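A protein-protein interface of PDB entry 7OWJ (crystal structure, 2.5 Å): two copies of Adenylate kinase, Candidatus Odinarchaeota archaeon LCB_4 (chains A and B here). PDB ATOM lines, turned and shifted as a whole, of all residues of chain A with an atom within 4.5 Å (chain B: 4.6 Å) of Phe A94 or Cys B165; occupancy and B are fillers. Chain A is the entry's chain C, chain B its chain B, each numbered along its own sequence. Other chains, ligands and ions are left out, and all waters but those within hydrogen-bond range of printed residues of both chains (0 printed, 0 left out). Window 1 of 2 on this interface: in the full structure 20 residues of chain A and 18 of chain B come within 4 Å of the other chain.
The side-chain amide nitrogen (NE2) of Gln B164 is in hydrogen-bond range of the side-chain hydroxyl (OH) of Tyr A95 (3.2 Å).
O of Val B167 lies within hydrogen-bond range of N of Phe A94 (2.7 Å).
O of Asp B109 lies within hydrogen-bond range of N of Tyr B166.
The backbone carbonyl oxygen (O) of Tyr B166 lies within hydrogen-bond range of the backbone NH (N) of Ile B111.
OG of Ser B160 lies within hydrogen-bond range of O of Cys B165.
O of Leu A88 sits at hydrogen-bond distance from N of Tyr A95 (2.9 Å).
Among the printed residues, pairs that only touch across the chains: Gly A93 with Tyr B166 (3.96 Å), Gly A93 with Val B167 (3.4 Å), Phe A94 with Cys B165 (3.98 Å), Phe A94 with Tyr B166 (3.2 Å), Tyr A95 with Cys B165 (3.9 Å), Tyr A95 with Tyr B166 (3.5 Å), Pro A96 with Ser B160 (3.4 Å), Pro A96 with Gln B164 (3.3 Å) and Pro A96 with Cys B165 (3.7 Å).
Printed residues of chain B within 4 Å of Phe A94: Cys B165, Tyr B166 and Val B167.
Of the printed residues of chain A, Cys B165 touches Phe A94, Tyr A95 and Pro A96.
Of the printed residues of chain A, Ser B160 touches Pro A96.
Of the printed residues of chain A, Tyr B166 touches Gly A93 (3.96 Å), Phe A94 (3.2 Å) and Tyr A95 (3.5 Å).
The nearest printed residue of chain B that does not touch Tyr A95 is Val B167 (5.1 Å).
Printed residues of chain B that touch a printed residue of chain A: Ser B160, Gln B164, Cys B165, Tyr B166 and Val B167.
Hydrophobic or aromatic side chains of chain B within 4 Å of the printed part of chain A: Tyr B166.
Of the 10 printed residues of chain A, 4 touch a printed residue of chain B.
No position is printed for both chains.
Of the 11 pairs that touch across the chains among the printed residues, none has its exchanged pair printed and touching as well.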
ATOM      1  N   SER A  87      12.814  -3.426  16.604  1.00  0.00           N
ATOM      2  CA  SER A  87      13.759  -4.133  15.756  1.00  0.00           C
ATOM      3  C   SER A  87      15.154  -3.654  16.086  1.00  0.00           C
ATOM      4  O   SER A  87      15.343  -2.599  16.704  1.00  0.00           O
ATOM      5  CB  SER A  87      13.527  -3.943  14.241  1.00  0.00           C
ATOM      6  OG  SER A  87      13.855  -2.630  13.800  1.00  0.00           O
ATOM      7  N   LEU A  88      16.116  -4.459  15.670  1.00  0.00           N
ATOM      8  CA  LEU A  88      17.508  -4.083  15.686  1.00  0.00           C
ATOM      9  C   LEU A  88      18.101  -4.399  14.335  1.00  0.00           C
ATOM     10  O   LEU A  88      17.699  -5.372  13.680  1.00  0.00           O
ATOM     11  CB  LEU A  88      18.238  -4.789  16.773  1.00  0.00           C
ATOM     12  CG  LEU A  88      17.689  -4.394  18.142  1.00  0.00           C
ATOM     13  CD1 LEU A  88      18.375  -5.259  19.176  1.00  0.00           C
ATOM     14  CD2 LEU A  88      17.841  -2.877  18.441  1.00  0.00           C
ATOM     15  N   LYS A  89      19.020  -3.534  13.922  1.00  0.00           N
ATOM     16  CA  LYS A  89      19.757  -3.685  12.681  1.00  0.00           C
ATOM     17  C   LYS A  89      20.889  -4.689  12.875  1.00  0.00           C
ATOM     18  O   LYS A  89      21.626  -4.612  13.854  1.00  0.00           O
ATOM     19  CB  LYS A  89      20.283  -2.310  12.247  1.00  0.00           C
ATOM     20  CG  LYS A  89      21.177  -2.266  11.038  1.00  0.00           C
ATOM     21  CD  LYS A  89      20.420  -2.181   9.746  1.00  0.00           C
ATOM     22  CE  LYS A  89      21.365  -1.912   8.579  1.00  0.00           C
ATOM     23  NZ  LYS A  89      22.598  -2.789   8.613  1.00  0.00           N
ATOM     24  N   GLY A  93      20.190  -7.689   8.250  1.00  0.00           N
ATOM     25  CA  GLY A  93      19.015  -6.845   8.179  1.00  0.00           C
ATOM     26  C   GLY A  93      18.302  -6.570   9.497  1.00  0.00           C
ATOM     27  O   GLY A  93      18.863  -6.814  10.571  1.00  0.00           O
ATOM     28  N   PHE A  94      17.060  -6.069   9.427  1.00  0.00           N
ATOM     29  CA  PHE A  94      16.269  -5.783  10.611  1.00  0.00           C
ATOM     30  C   PHE A  94      15.720  -7.062  11.216  1.00  0.00           C
ATOM     31  O   PHE A  94      15.276  -7.965  10.507  1.00  0.00           O
ATOM     32  CB  PHE A  94      15.146  -4.814  10.250  1.00  0.00           C
ATOM     33  CG  PHE A  94      15.649  -3.463   9.904  1.00  0.00           C
ATOM     34  CD1 PHE A  94      16.071  -2.590  10.883  1.00  0.00           C
ATOM     35  CD2 PHE A  94      15.778  -3.091   8.613  1.00  0.00           C
ATOM     36  CE1 PHE A  94      16.581  -1.362  10.561  1.00  0.00           C
ATOM     37  CE2 PHE A  94      16.299  -1.887   8.291  1.00  0.00           C
ATOM     38  CZ  PHE A  94      16.696  -1.012   9.248  1.00  0.00           C
ATOM     39  N   TYR A  95      15.806  -7.170  12.536  1.00  0.00           N
ATOM     40  CA  TYR A  95      15.255  -8.350  13.207  1.00  0.00           C
ATOM     41  C   TYR A  95      14.337  -7.926  14.346  1.00  0.00           C
ATOM     42  O   TYR A  95      14.656  -6.973  15.065  1.00  0.00           O
ATOM     43  CB  TYR A  95      16.361  -9.241  13.769  1.00  0.00           C
ATOM     44  CG  TYR A  95      15.906 -10.609  14.155  1.00  0.00           C
ATOM     45  CD1 TYR A  95      15.780 -11.601  13.210  1.00  0.00           C
ATOM     46  CD2 TYR A  95      15.616 -10.923  15.474  1.00  0.00           C
ATOM     47  CE1 TYR A  95      15.356 -12.852  13.556  1.00  0.00           C
ATOM     48  CE2 TYR A  95      15.209 -12.195  15.838  1.00  0.00           C
ATOM     49  CZ  TYR A  95      15.083 -13.151  14.875  1.00  0.00           C
ATOM     50  OH  TYR A  95      14.680 -14.421  15.215  1.00  0.00           O
ATOM     51  N   PRO A  96      13.205  -8.601  14.541  1.00  0.00           N
ATOM     52  CA  PRO A  96      12.261  -8.170  15.585  1.00  0.00           C
ATOM     53  C   PRO A  96      12.753  -8.499  17.002  1.00  0.00           C
ATOM     54  O   PRO A  96      13.342  -9.546  17.247  1.00  0.00           O
ATOM     55  CB  PRO A  96      10.978  -8.957  15.258  1.00  0.00           C
ATOM     56  CG  PRO A  96      11.219  -9.740  14.049  1.00  0.00           C
ATOM     57  CD  PRO A  96      12.712  -9.790  13.828  1.00  0.00           C
ATOM     58  N   LEU A 147      14.852   5.077   7.974  1.00  0.00           N
ATOM     59  CA  LEU A 147      14.397   3.760   7.580  1.00  0.00           C
ATOM     60  C   LEU A 147      14.085   2.922   8.803  1.00  0.00           C
ATOM     61  O   LEU A 147      13.079   2.188   8.849  1.00  0.00           O
ATOM     62  CB  LEU A 147      15.484   3.114   6.724  1.00  0.00           C
ATOM     63  CG  LEU A 147      15.397   1.653   6.313  1.00  0.00           C
ATOM     64  CD1 LEU A 147      14.114   1.423   5.547  1.00  0.00           C
ATOM     65  CD2 LEU A 147      16.551   1.242   5.508  1.00  0.00           C
ATOM     66  N   HIS A 148      14.955   2.988   9.794  1.00  0.00           N
ATOM     67  CA  HIS A 148      14.731   2.189  10.984  1.00  0.00           C
ATOM     68  C   HIS A 148      13.418   2.603  11.647  1.00  0.00           C
ATOM     69  O   HIS A 148      12.601   1.741  11.988  1.00  0.00           O
ATOM     70  CB  HIS A 148      15.945   2.301  11.922  1.00  0.00           C
ATOM     71  CG  HIS A 148      15.982   1.269  12.999  1.00  0.00           C
ATOM     72  ND1 HIS A 148      17.007   1.192  13.912  1.00  0.00           N
ATOM     73  CD2 HIS A 148      15.093   0.300  13.340  1.00  0.00           C
ATOM     74  CE1 HIS A 148      16.751   0.214  14.765  1.00  0.00           C
ATOM     75  NE2 HIS A 148      15.599  -0.348  14.436  1.00  0.00           N
ATOM     76  N   VAL A 151      10.521   1.200   9.815  1.00  0.00           N
ATOM     77  CA  VAL A 151      10.367  -0.241  10.053  1.00  0.00           C
ATOM     78  C   VAL A 151       9.707  -0.500  11.413  1.00  0.00           C
ATOM     79  O   VAL A 151       8.769  -1.304  11.524  1.00  0.00           O
ATOM     80  CB  VAL A 151      11.737  -0.947   9.933  1.00  0.00           C
ATOM     81  CG1 VAL A 151      11.755  -2.354  10.595  1.00  0.00           C
ATOM     82  CG2 VAL A 151      12.152  -1.038   8.482  1.00  0.00           C
ATOM     83  N   PRO B 108      12.820 -19.593   5.805  1.00  0.00           N
ATOM     84  CA  PRO B 108      13.955 -18.727   5.484  1.00  0.00           C
ATOM     85  C   PRO B 108      14.468 -17.988   6.705  1.00  0.00           C
ATOM     86  O   PRO B 108      13.708 -17.674   7.631  1.00  0.00           O
ATOM     87  CB  PRO B 108      13.363 -17.741   4.464  1.00  0.00           C
ATOM     88  CG  PRO B 108      11.882 -17.772   4.807  1.00  0.00           C
ATOM     89  CD  PRO B 108      11.594 -19.181   5.093  1.00  0.00           C
ATOM     90  N   ASP B 109      15.767 -17.664   6.661  1.00  0.00           N
ATOM     91  CA  ASP B 109      16.372 -16.775   7.652  1.00  0.00           C
ATOM     92  C   ASP B 109      15.981 -15.317   7.442  1.00  0.00           C
ATOM     93  O   ASP B 109      15.944 -14.559   8.400  1.00  0.00           O
ATOM     94  CB  ASP B 109      17.896 -16.924   7.617  1.00  0.00           C
ATOM     95  CG  ASP B 109      18.363 -18.412   7.758  1.00  0.00           C
ATOM     96  OD1 ASP B 109      18.229 -19.001   8.867  1.00  0.00           O
ATOM     97  OD2 ASP B 109      18.859 -18.996   6.753  1.00  0.00           O
ATOM     98  N   GLY B 110      15.681 -14.899   6.216  1.00  0.00           N
ATOM     99  CA  GLY B 110      15.255 -13.523   6.036  1.00  0.00           C
ATOM    100  C   GLY B 110      14.755 -13.266   4.638  1.00  0.00           C
ATOM    101  O   GLY B 110      14.787 -14.143   3.766  1.00  0.00           O
ATOM    102  N   ILE B 111      14.290 -12.029   4.448  1.00  0.00           N
ATOM    103  CA  ILE B 111      13.807 -11.512   3.170  1.00  0.00           C
ATOM    104  C   ILE B 111      14.711 -10.372   2.726  1.00  0.00           C
ATOM    105  O   ILE B 111      15.015  -9.465   3.512  1.00  0.00           O
ATOM    106  CB  ILE B 111      12.359 -11.011   3.268  1.00  0.00           C
ATOM    107  CG1 ILE B 111      11.478 -12.048   3.979  1.00  0.00           C
ATOM    108  CG2 ILE B 111      11.860 -10.749   1.910  1.00  0.00           C
ATOM    109  CD1 ILE B 111       9.983 -11.671   4.165  1.00  0.00           C
ATOM    110  N   TYR B 159       5.542 -10.239   7.334  1.00  0.00           N
ATOM    111  CA  TYR B 159       6.020 -11.609   7.364  1.00  0.00           C
ATOM    112  C   TYR B 159       7.090 -11.778   8.425  1.00  0.00           C
ATOM    113  O   TYR B 159       7.168 -12.842   9.041  1.00  0.00           O
ATOM    114  CB  TYR B 159       6.549 -12.026   5.998  1.00  0.00           C
ATOM    115  CG  TYR B 159       5.498 -12.104   4.943  1.00  0.00           C
ATOM    116  CD1 TYR B 159       4.462 -12.980   5.055  1.00  0.00           C
ATOM    117  CD2 TYR B 159       5.556 -11.298   3.796  1.00  0.00           C
ATOM    118  CE1 TYR B 159       3.496 -13.051   4.079  1.00  0.00           C
ATOM    119  CE2 TYR B 159       4.581 -11.382   2.812  1.00  0.00           C
ATOM    120  CZ  TYR B 159       3.569 -12.251   2.971  1.00  0.00           C
ATOM    121  OH  TYR B 159       2.607 -12.351   2.038  1.00  0.00           O
ATOM    122  N   SER B 160       7.888 -10.727   8.675  1.00  0.00           N
ATOM    123  CA  SER B 160       8.888 -10.789   9.735  1.00  0.00           C
ATOM    124  C   SER B 160       8.234 -10.827  11.115  1.00  0.00           C
ATOM    125  O   SER B 160       8.678 -11.566  12.004  1.00  0.00           O
ATOM    126  CB  SER B 160       9.837  -9.597   9.630  1.00  0.00           C
ATOM    127  OG  SER B 160      10.749  -9.507  10.717  1.00  0.00           O
ATOM    128  N   ASN B 163       6.754 -14.504  11.449  1.00  0.00           N
ATOM    129  CA  ASN B 163       7.670 -15.668  11.320  1.00  0.00           C
ATOM    130  C   ASN B 163       9.055 -15.480  11.926  1.00  0.00           C
ATOM    131  O   ASN B 163       9.824 -16.407  11.817  1.00  0.00           O
ATOM    132  CB  ASN B 163       7.888 -16.025   9.855  1.00  0.00           C
ATOM    133  CG  ASN B 163       6.605 -16.371   9.147  1.00  0.00           C
ATOM    134  OD1 ASN B 163       5.984 -17.367   9.444  1.00  0.00           O
ATOM    135  ND2 ASN B 163       6.131 -15.503   8.282  1.00  0.00           N
ATOM    136  N   GLN B 164       9.335 -14.364  12.581  1.00  0.00           N
ATOM    137  CA  GLN B 164      10.642 -14.039  13.217  1.00  0.00           C
ATOM    138  C   GLN B 164      11.817 -14.180  12.246  1.00  0.00           C
ATOM    139  O   GLN B 164      12.712 -14.925  12.546  1.00  0.00           O
ATOM    140  CB  GLN B 164      10.911 -14.877  14.466  1.00  0.00           C
ATOM    141  CG  GLN B 164      10.221 -14.320  15.686  1.00  0.00           C
ATOM    142  CD  GLN B 164      11.048 -13.238  16.316  1.00  0.00           C
ATOM    143  OE1 GLN B 164      10.697 -12.077  16.267  1.00  0.00           O
ATOM    144  NE2 GLN B 164      12.143 -13.621  16.934  1.00  0.00           N
ATOM    145  N   CYS B 165      11.807 -13.504  11.115  1.00  0.00           N
ATOM    146  CA  CYS B 165      12.907 -13.575  10.127  1.00  0.00           C
ATOM    147  C   CYS B 165      13.548 -12.197   9.960  1.00  0.00           C
ATOM    148  O   CYS B 165      13.029 -11.255  10.489  1.00  0.00           O
ATOM    149  CB  CYS B 165      12.372 -14.136   8.821  1.00  0.00           C
ATOM    150  SG  CYS B 165      11.312 -12.995   7.913  1.00  0.00           S
ATOM    151  N   TYR B 166      14.690 -12.113   9.301  1.00  0.00           N
ATOM    152  CA  TYR B 166      15.360 -10.844   9.032  1.00  0.00           C
ATOM    153  C   TYR B 166      14.665 -10.112   7.881  1.00  0.00           C
ATOM    154  O   TYR B 166      13.920 -10.695   7.102  1.00  0.00           O
ATOM    155  CB  TYR B 166      16.837 -11.053   8.692  1.00  0.00           C
ATOM    156  CG  TYR B 166      17.704 -11.574   9.833  1.00  0.00           C
ATOM    157  CD1 TYR B 166      18.192 -10.714  10.816  1.00  0.00           C
ATOM    158  CD2 TYR B 166      18.089 -12.909   9.890  1.00  0.00           C
ATOM    159  CE1 TYR B 166      18.998 -11.169  11.848  1.00  0.00           C
ATOM    160  CE2 TYR B 166      18.912 -13.369  10.912  1.00  0.00           C
ATOM    161  CZ  TYR B 166      19.353 -12.488  11.895  1.00  0.00           C
ATOM    162  OH  TYR B 166      20.154 -12.913  12.927  1.00  0.00           O
ATOM    163  N   VAL B 167      14.886  -8.811   7.813  1.00  0.00           N
ATOM    164  CA  VAL B 167      14.361  -7.976   6.738  1.00  0.00           C
ATOM    165  C   VAL B 167      15.494  -7.066   6.305  1.00  0.00           C
ATOM    166  O   VAL B 167      15.876  -6.165   7.057  1.00  0.00           O
ATOM    167  CB  VAL B 167      13.159  -7.131   7.158  1.00  0.00           C
ATOM    168  CG1 VAL B 167      12.636  -6.408   5.944  1.00  0.00           C
ATOM    169  CG2 VAL B 167      12.114  -7.994   7.788  1.00  0.00           C
